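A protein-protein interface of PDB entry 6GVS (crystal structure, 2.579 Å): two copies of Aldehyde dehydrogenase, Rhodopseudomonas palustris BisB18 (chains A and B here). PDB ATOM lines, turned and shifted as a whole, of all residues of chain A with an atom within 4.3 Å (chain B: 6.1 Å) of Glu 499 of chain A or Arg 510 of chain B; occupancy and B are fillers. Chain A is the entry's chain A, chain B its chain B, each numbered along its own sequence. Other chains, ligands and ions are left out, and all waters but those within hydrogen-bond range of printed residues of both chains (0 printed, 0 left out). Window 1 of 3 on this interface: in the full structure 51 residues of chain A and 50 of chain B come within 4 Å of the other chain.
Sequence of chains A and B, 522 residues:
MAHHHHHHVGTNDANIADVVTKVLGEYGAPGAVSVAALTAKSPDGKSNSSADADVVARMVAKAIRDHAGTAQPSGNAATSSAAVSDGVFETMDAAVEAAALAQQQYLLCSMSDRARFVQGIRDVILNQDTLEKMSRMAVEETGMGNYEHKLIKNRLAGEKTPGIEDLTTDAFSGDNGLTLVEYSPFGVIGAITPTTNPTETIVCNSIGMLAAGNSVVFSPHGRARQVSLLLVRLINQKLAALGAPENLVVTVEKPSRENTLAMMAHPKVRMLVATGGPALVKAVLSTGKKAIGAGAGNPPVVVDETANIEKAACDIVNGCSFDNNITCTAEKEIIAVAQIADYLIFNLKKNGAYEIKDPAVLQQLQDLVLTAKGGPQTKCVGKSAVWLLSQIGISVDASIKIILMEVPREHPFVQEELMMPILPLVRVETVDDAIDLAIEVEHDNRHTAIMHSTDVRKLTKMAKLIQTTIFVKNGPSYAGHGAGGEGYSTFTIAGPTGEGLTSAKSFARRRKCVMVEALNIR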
ATOM      1  N   LYS A 290       4.709 -34.024 -24.695  1.00  0.00           N
ATOM      2  CA  LYS A 290       4.335 -32.872 -23.887  1.00  0.00           C
ATOM      3  C   LYS A 290       4.278 -33.286 -22.424  1.00  0.00           C
ATOM      4  O   LYS A 290       3.674 -34.306 -22.080  1.00  0.00           O
ATOM      5  CB  LYS A 290       2.980 -32.333 -24.349  1.00  0.00           C
ATOM      6  CG  LYS A 290       2.363 -31.268 -23.452  1.00  0.00           C
ATOM      7  CD  LYS A 290       3.156 -29.974 -23.473  1.00  0.00           C
ATOM      8  CE  LYS A 290       2.391 -28.858 -22.773  1.00  0.00           C
ATOM      9  NZ  LYS A 290       3.187 -27.606 -22.668  1.00  0.00           N
ATOM     10  N   ILE A 292       4.168 -31.657 -18.249  1.00  0.00           N
ATOM     11  CA  ILE A 292       4.155 -30.641 -17.204  1.00  0.00           C
ATOM     12  C   ILE A 292       4.942 -31.191 -16.024  1.00  0.00           C
ATOM     13  O   ILE A 292       4.658 -32.296 -15.543  1.00  0.00           O
ATOM     14  CB  ILE A 292       2.719 -30.277 -16.792  1.00  0.00           C
ATOM     15  CG1 ILE A 292       1.966 -29.666 -17.980  1.00  0.00           C
ATOM     16  CG2 ILE A 292       2.730 -29.323 -15.600  1.00  0.00           C
ATOM     17  CD1 ILE A 292       0.520 -29.320 -17.686  1.00  0.00           C
ATOM     18  N   THR A 469       7.444 -19.282  -8.497  1.00  0.00           N
ATOM     19  CA  THR A 469       6.084 -19.511  -8.970  1.00  0.00           C
ATOM     20  C   THR A 469       5.049 -19.043  -7.955  1.00  0.00           C
ATOM     21  O   THR A 469       3.973 -18.573  -8.336  1.00  0.00           O
ATOM     22  CB  THR A 469       5.873 -20.995  -9.279  1.00  0.00           C
ATOM     23  OG1 THR A 469       6.772 -21.407 -10.315  1.00  0.00           O
ATOM     24  CG2 THR A 469       4.442 -21.252  -9.722  1.00  0.00           C
ATOM     25  N   ALA A 494       3.825 -26.133 -11.131  1.00  0.00           N
ATOM     26  CA  ALA A 494       4.829 -26.341 -12.170  1.00  0.00           C
ATOM     27  C   ALA A 494       5.710 -25.102 -12.291  1.00  0.00           C
ATOM     28  O   ALA A 494       5.344 -24.124 -12.948  1.00  0.00           O
ATOM     29  CB  ALA A 494       4.155 -26.665 -13.502  1.00  0.00           C
ATOM     30  N   THR A 497       8.377 -26.174 -15.968  1.00  0.00           N
ATOM     31  CA  THR A 497       7.702 -26.084 -17.257  1.00  0.00           C
ATOM     32  C   THR A 497       6.875 -24.813 -17.415  1.00  0.00           C
ATOM     33  O   THR A 497       6.387 -24.551 -18.519  1.00  0.00           O
ATOM     34  CB  THR A 497       6.813 -27.314 -17.476  1.00  0.00           C
ATOM     35  OG1 THR A 497       6.055 -27.593 -16.292  1.00  0.00           O
ATOM     36  CG2 THR A 497       7.659 -28.532 -17.839  1.00  0.00           C
ATOM     37  N   GLY A 498       6.694 -24.031 -16.352  1.00  0.00           N
ATOM     38  CA  GLY A 498       6.173 -22.684 -16.471  1.00  0.00           C
ATOM     39  C   GLY A 498       4.671 -22.525 -16.368  1.00  0.00           C
ATOM     40  O   GLY A 498       4.186 -21.384 -16.408  1.00  0.00           O
ATOM     41  N   GLU A 499       3.916 -23.615 -16.219  1.00  0.00           N
ATOM     42  CA  GLU A 499       2.463 -23.516 -16.204  1.00  0.00           C
ATOM     43  C   GLU A 499       1.912 -22.922 -14.913  1.00  0.00           C
ATOM     44  O   GLU A 499       0.721 -22.594 -14.868  1.00  0.00           O
ATOM     45  CB  GLU A 499       1.841 -24.897 -16.436  1.00  0.00           C
ATOM     46  CG  GLU A 499       2.098 -25.481 -17.826  1.00  0.00           C
ATOM     47  CD  GLU A 499       3.453 -26.160 -17.945  1.00  0.00           C
ATOM     48  OE1 GLU A 499       4.193 -26.183 -16.937  1.00  0.00           O
ATOM     49  OE2 GLU A 499       3.774 -26.674 -19.043  1.00  0.00           O
ATOM     50  N   GLY A 500       2.721 -22.779 -13.869  1.00  0.00           N
ATOM     51  CA  GLY A 500       2.253 -22.199 -12.634  1.00  0.00           C
ATOM     52  C   GLY A 500       1.367 -23.130 -11.838  1.00  0.00           C
ATOM     53  O   GLY A 500       1.603 -24.344 -11.809  1.00  0.00           O
ATOM     54  N   LEU A 501       0.350 -22.577 -11.186  1.00  0.00           N
ATOM     55  CA  LEU A 501      -0.613 -23.373 -10.430  1.00  0.00           C
ATOM     56  C   LEU A 501      -1.573 -24.033 -11.413  1.00  0.00           C
ATOM     57  O   LEU A 501      -2.523 -23.408 -11.887  1.00  0.00           O
ATOM     58  CB  LEU A 501      -1.360 -22.501  -9.429  1.00  0.00           C
ATOM     59  CG  LEU A 501      -0.609 -22.164  -8.139  1.00  0.00           C
ATOM     60  CD1 LEU A 501       0.344 -20.998  -8.351  1.00  0.00           C
ATOM     61  CD2 LEU A 501      -1.587 -21.875  -7.003  1.00  0.00           C
ATOM     62  N   ASP B 170      -3.204 -10.856 -14.320  1.00  0.00           N
ATOM     63  CA  ASP B 170      -4.453 -11.249 -13.685  1.00  0.00           C
ATOM     64  C   ASP B 170      -4.433 -10.839 -12.219  1.00  0.00           C
ATOM     65  O   ASP B 170      -3.381 -10.814 -11.575  1.00  0.00           O
ATOM     66  CB  ASP B 170      -4.682 -12.754 -13.804  1.00  0.00           C
ATOM     67  CG  ASP B 170      -4.917 -13.189 -15.230  1.00  0.00           C
ATOM     68  OD1 ASP B 170      -5.356 -12.341 -16.040  1.00  0.00           O
ATOM     69  OD2 ASP B 170      -4.661 -14.372 -15.540  1.00  0.00           O
ATOM     70  N   VAL B 181      -1.074 -12.387 -10.892  1.00  0.00           N
ATOM     71  CA  VAL B 181      -0.467 -13.434 -11.706  1.00  0.00           C
ATOM     72  C   VAL B 181       0.209 -12.756 -12.888  1.00  0.00           C
ATOM     73  O   VAL B 181      -0.446 -12.046 -13.662  1.00  0.00           O
ATOM     74  CB  VAL B 181      -1.494 -14.476 -12.183  1.00  0.00           C
ATOM     75  CG1 VAL B 181      -0.791 -15.645 -12.872  1.00  0.00           C
ATOM     76  CG2 VAL B 181      -2.330 -14.969 -11.011  1.00  0.00           C
ATOM     77  N   GLU B 182       1.512 -12.981 -13.030  1.00  0.00           N
ATOM     78  CA  GLU B 182       2.332 -12.273 -13.999  1.00  0.00           C
ATOM     79  C   GLU B 182       3.065 -13.268 -14.887  1.00  0.00           C
ATOM     80  O   GLU B 182       3.219 -14.443 -14.550  1.00  0.00           O
ATOM     81  CB  GLU B 182       3.351 -11.359 -13.296  1.00  0.00           C
ATOM     82  CG  GLU B 182       2.738 -10.329 -12.354  1.00  0.00           C
ATOM     83  CD  GLU B 182       2.333  -9.050 -13.067  1.00  0.00           C
ATOM     84  OE1 GLU B 182       2.423  -7.966 -12.451  1.00  0.00           O
ATOM     85  OE2 GLU B 182       1.931  -9.126 -14.247  1.00  0.00           O
ATOM     86  N   TYR B 183       3.515 -12.772 -16.038  1.00  0.00           N
ATOM     87  CA  TYR B 183       4.344 -13.537 -16.961  1.00  0.00           C
ATOM     88  C   TYR B 183       5.793 -13.095 -16.790  1.00  0.00           C
ATOM     89  O   TYR B 183       6.125 -11.940 -17.073  1.00  0.00           O
ATOM     90  CB  TYR B 183       3.898 -13.328 -18.407  1.00  0.00           C
ATOM     91  CG  TYR B 183       2.542 -13.907 -18.739  1.00  0.00           C
ATOM     92  CD1 TYR B 183       2.388 -15.262 -19.000  1.00  0.00           C
ATOM     93  CD2 TYR B 183       1.419 -13.095 -18.811  1.00  0.00           C
ATOM     94  CE1 TYR B 183       1.154 -15.794 -19.310  1.00  0.00           C
ATOM     95  CE2 TYR B 183       0.181 -13.618 -19.122  1.00  0.00           C
ATOM     96  CZ  TYR B 183       0.056 -14.967 -19.373  1.00  0.00           C
ATOM     97  OH  TYR B 183      -1.174 -15.499 -19.679  1.00  0.00           O
ATOM     98  N   SER B 184       6.646 -14.004 -16.339  1.00  0.00           N
ATOM     99  CA  SER B 184       8.045 -13.701 -16.080  1.00  0.00           C
ATOM    100  C   SER B 184       8.959 -14.497 -17.002  1.00  0.00           C
ATOM    101  O   SER B 184       8.548 -15.510 -17.580  1.00  0.00           O
ATOM    102  CB  SER B 184       8.403 -13.993 -14.617  1.00  0.00           C
ATOM    103  OG  SER B 184       8.040 -12.905 -13.785  1.00  0.00           O
ATOM    104  N   LYS B 290      12.070 -27.971 -20.971  1.00  0.00           N
ATOM    105  CA  LYS B 290      10.820 -27.403 -21.457  1.00  0.00           C
ATOM    106  C   LYS B 290      10.943 -27.145 -22.950  1.00  0.00           C
ATOM    107  O   LYS B 290      11.939 -26.577 -23.411  1.00  0.00           O
ATOM    108  CB  LYS B 290      10.499 -26.109 -20.714  1.00  0.00           C
ATOM    109  CG  LYS B 290       9.316 -25.326 -21.279  1.00  0.00           C
ATOM    110  CD  LYS B 290       8.001 -26.079 -21.138  1.00  0.00           C
ATOM    111  CE  LYS B 290       6.830 -25.254 -21.668  1.00  0.00           C
ATOM    112  NZ  LYS B 290       5.557 -26.032 -21.710  1.00  0.00           N
ATOM    113  N   GLU B 499       0.416 -25.089 -27.226  1.00  0.00           N
ATOM    114  CA  GLU B 499       0.471 -23.657 -26.971  1.00  0.00           C
ATOM    115  C   GLU B 499      -0.352 -22.857 -27.975  1.00  0.00           C
ATOM    116  O   GLU B 499      -0.682 -21.699 -27.701  1.00  0.00           O
ATOM    117  CB  GLU B 499       1.919 -23.168 -26.988  1.00  0.00           C
ATOM    118  CG  GLU B 499       2.737 -23.607 -25.788  1.00  0.00           C
ATOM    119  CD  GLU B 499       3.226 -25.035 -25.901  1.00  0.00           C
ATOM    120  OE1 GLU B 499       3.081 -25.625 -26.990  1.00  0.00           O
ATOM    121  OE2 GLU B 499       3.763 -25.566 -24.902  1.00  0.00           O
ATOM    122  N   LYS B 505       3.505 -14.514 -24.359  1.00  0.00           N
ATOM    123  CA  LYS B 505       3.053 -15.357 -23.258  1.00  0.00           C
ATOM    124  C   LYS B 505       3.654 -16.756 -23.339  1.00  0.00           C
ATOM    125  O   LYS B 505       3.980 -17.362 -22.313  1.00  0.00           O
ATOM    126  CB  LYS B 505       1.524 -15.457 -23.265  1.00  0.00           C
ATOM    127  CG  LYS B 505       0.778 -14.233 -22.749  1.00  0.00           C
ATOM    128  CD  LYS B 505      -0.720 -14.535 -22.595  1.00  0.00           C
ATOM    129  CE  LYS B 505      -1.564 -13.953 -23.728  1.00  0.00           C
ATOM    130  NZ  LYS B 505      -2.055 -12.574 -23.420  1.00  0.00           N
ATOM    131  N   ALA B 508       7.037 -17.418 -21.426  1.00  0.00           N
ATOM    132  CA  ALA B 508       7.090 -16.891 -20.072  1.00  0.00           C
ATOM    133  C   ALA B 508       6.543 -17.917 -19.088  1.00  0.00           C
ATOM    134  O   ALA B 508       5.711 -18.757 -19.440  1.00  0.00           O
ATOM    135  CB  ALA B 508       6.292 -15.583 -19.955  1.00  0.00           C
ATOM    136  N   ARG B 509       7.027 -17.839 -17.851  1.00  0.00           N
ATOM    137  CA  ARG B 509       6.507 -18.642 -16.755  1.00  0.00           C
ATOM    138  C   ARG B 509       5.439 -17.854 -16.005  1.00  0.00           C
ATOM    139  O   ARG B 509       5.518 -16.631 -15.877  1.00  0.00           O
ATOM    140  CB  ARG B 509       7.624 -19.043 -15.787  1.00  0.00           C
ATOM    141  CG  ARG B 509       8.844 -19.650 -16.466  1.00  0.00           C
ATOM    142  CD  ARG B 509       9.815 -20.288 -15.471  1.00  0.00           C
ATOM    143  NE  ARG B 509      10.165 -19.400 -14.367  1.00  0.00           N
ATOM    144  CZ  ARG B 509       9.615 -19.451 -13.155  1.00  0.00           C
ATOM    145  NH1 ARG B 509       8.678 -20.347 -12.871  1.00  0.00           N
ATOM    146  NH2 ARG B 509      10.007 -18.595 -12.219  1.00  0.00           N
ATOM    147  N   ARG B 510       4.432 -18.565 -15.510  1.00  0.00           N
ATOM    148  CA  ARG B 510       3.397 -17.947 -14.692  1.00  0.00           C
ATOM    149  C   ARG B 510       3.849 -17.939 -13.237  1.00  0.00           C
ATOM    150  O   ARG B 510       4.295 -18.964 -12.710  1.00  0.00           O
ATOM    151  CB  ARG B 510       2.063 -18.680 -14.842  1.00  0.00           C
ATOM    152  CG  ARG B 510       1.385 -18.433 -16.185  1.00  0.00           C
ATOM    153  CD  ARG B 510       0.036 -19.126 -16.299  1.00  0.00           C
ATOM    154  NE  ARG B 510      -1.038 -18.369 -15.658  1.00  0.00           N
ATOM    155  CZ  ARG B 510      -1.562 -17.245 -16.145  1.00  0.00           C
ATOM    156  NH1 ARG B 510      -2.542 -16.628 -15.501  1.00  0.00           N
ATOM    157  NH2 ARG B 510      -1.097 -16.731 -17.275  1.00  0.00           N
ATOM    158  N   ARG B 511       3.754 -16.774 -12.602  1.00  0.00           N
ATOM    159  CA  ARG B 511       4.089 -16.621 -11.195  1.00  0.00           C
ATOM    160  C   ARG B 511       2.905 -16.002 -10.467  1.00  0.00           C
ATOM    161  O   ARG B 511       2.124 -15.245 -11.048  1.00  0.00           O
ATOM    162  CB  ARG B 511       5.341 -15.756 -10.998  1.00  0.00           C
ATOM    163  CG  ARG B 511       6.594 -16.330 -11.641  1.00  0.00           C
ATOM    164  CD  ARG B 511       7.863 -15.624 -11.155  1.00  0.00           C
ATOM    165  NE  ARG B 511       7.668 -14.185 -11.001  1.00  0.00           N
ATOM    166  CZ  ARG B 511       7.812 -13.511  -9.860  1.00  0.00           C
ATOM    167  NH1 ARG B 511       8.175 -14.125  -8.742  1.00  0.00           N
ATOM    168  NH2 ARG B 511       7.602 -12.203  -9.842  1.00  0.00           N
ATOM    169  N   LYS B 512       2.784 -16.335  -9.186  1.00  0.00           N
ATOM    170  CA  LYS B 512       1.674 -15.903  -8.348  1.00  0.00           C
ATOM    171  C   LYS B 512       2.231 -15.161  -7.143  1.00  0.00           C
ATOM    172  O   LYS B 512       3.151 -15.649  -6.479  1.00  0.00           O
ATOM    173  CB  LYS B 512       0.832 -17.101  -7.904  1.00  0.00           C
ATOM    174  CG  LYS B 512      -0.366 -16.761  -7.028  1.00  0.00           C
ATOM    175  CD  LYS B 512      -1.052 -18.033  -6.529  1.00  0.00           C
ATOM    176  CE  LYS B 512      -2.278 -17.720  -5.681  1.00  0.00           C
ATOM    177  NZ  LYS B 512      -2.894 -18.951  -5.111  1.00  0.00           N
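The side-chain amino group (NZ) of Lys 290 of chain A is in salt-bridge range of the side-chain carboxylate (OE2) of Glu 499 of chain B, at 3.1 Å.
OG1 of Thr 469 of chain A is in hydrogen-bond range of NH1 of Arg 509 of chain B.
O of Thr 469 of chain A is in hydrogen-bond range of N of Lys 512 of chain B, at 2.7 Å.
N of Arg 510 of chain B is in hydrogen-bond range of O of Gly 498 of chain A.
NZ of Lys 290 of chain B lies within salt-bridge range of OE2 of Glu 499 of chain A, at 3.3 Å.
NZ of Lys 290 of chain A sits close to NZ of Lys 290 of chain B.
The side-chain amino group (NZ) of Lys 290 of chain A lies within salt-bridge range of the side-chain carboxylate (OE2) of Glu 499 of chain A (3.8 Å).
N of Ala 494 of chain A sits at hydrogen-bond distance from O of Gly 500 of chain A (2.9 Å).
The side-chain carboxylate (OD2) of Asp 170 of chain B lies within salt-bridge range of the guanidinium group (NH1) of Arg 510 of chain B (3.1 Å).
The backbone NH of Glu 182 of chain B sits at hydrogen-bond distance from the backbone carbonyl oxygen of Arg 511 of chain B (3.1 Å).
The backbone carbonyl oxygen (O) of Ser 184 of chain B sits at hydrogen-bond distance from the backbone NH (N) of Arg 509 of chain B.
The side-chain carboxylate of Glu 499 of chain B is in salt-bridge range of the side-chain amino group of Lys 290 of chain B, 3.7 Å away.
CG2 of Thr 469 of chain A touches O of Arg 510 of chain B (3.8 Å).
O of Thr 469 of chain A touches CA of Arg 511 of chain B, 3.5 Å away.
Lys 290 of chain B touches Thr 497 of chain A.
Gly 498 of chain A touches Arg 509 of chain B.
Arg 510 of chain B touches Glu 499 of chain A (CD to O, 3.8 Å).
Arg 510 of chain B touches Gly 500 of chain A (O to CA, 3.8 Å).
Leu 501 of chain A touches Lys 512 of chain B (CD2 to NZ, 3.7 Å).
Glu 499 of chain A touches just these residues of chain B: Lys 290 (3.3 Å) and Arg 510 (3.8 Å).
Of chain A, only Thr 469, Gly 498, Glu 499 and Gly 500 come within 4 Å of Arg 510 of chain B.
Of the printed residues of chain A, Arg 511 of chain B touches Thr 469.
Of the printed residues of chain A, Lys 290 of chain B touches Lys 290, Thr 497 and Glu 499.
Of the printed residues of chain A, Arg 509 of chain B touches Thr 469 and Gly 498.
The nearest residue of chain B that does not touch Glu 499 of chain A is Arg 509 of chain B (5.6 Å).
The nearest printed residue of chain A that does not touch Arg 510 of chain B is Ala 494 of chain A (5.3 Å).
The nearest printed residue of chain A that does not touch Arg 509 of chain B is Ala 494 of chain A (5.0 Å).
Printed residues of chain A that touch a printed residue of chain B: Lys 290, Thr 469, Thr 497, Gly 498, Glu 499, Gly 500 and Leu 501.
Lys 290 of chain A touches its own counterpart, Lys 290 of chain B.
Lys 290 of chain A touches Glu 499 of chain B, and with the chains exchanged Glu 499 of chain A touches Lys 290 of chain B.
Positions printed for both chains: 290 and 499.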
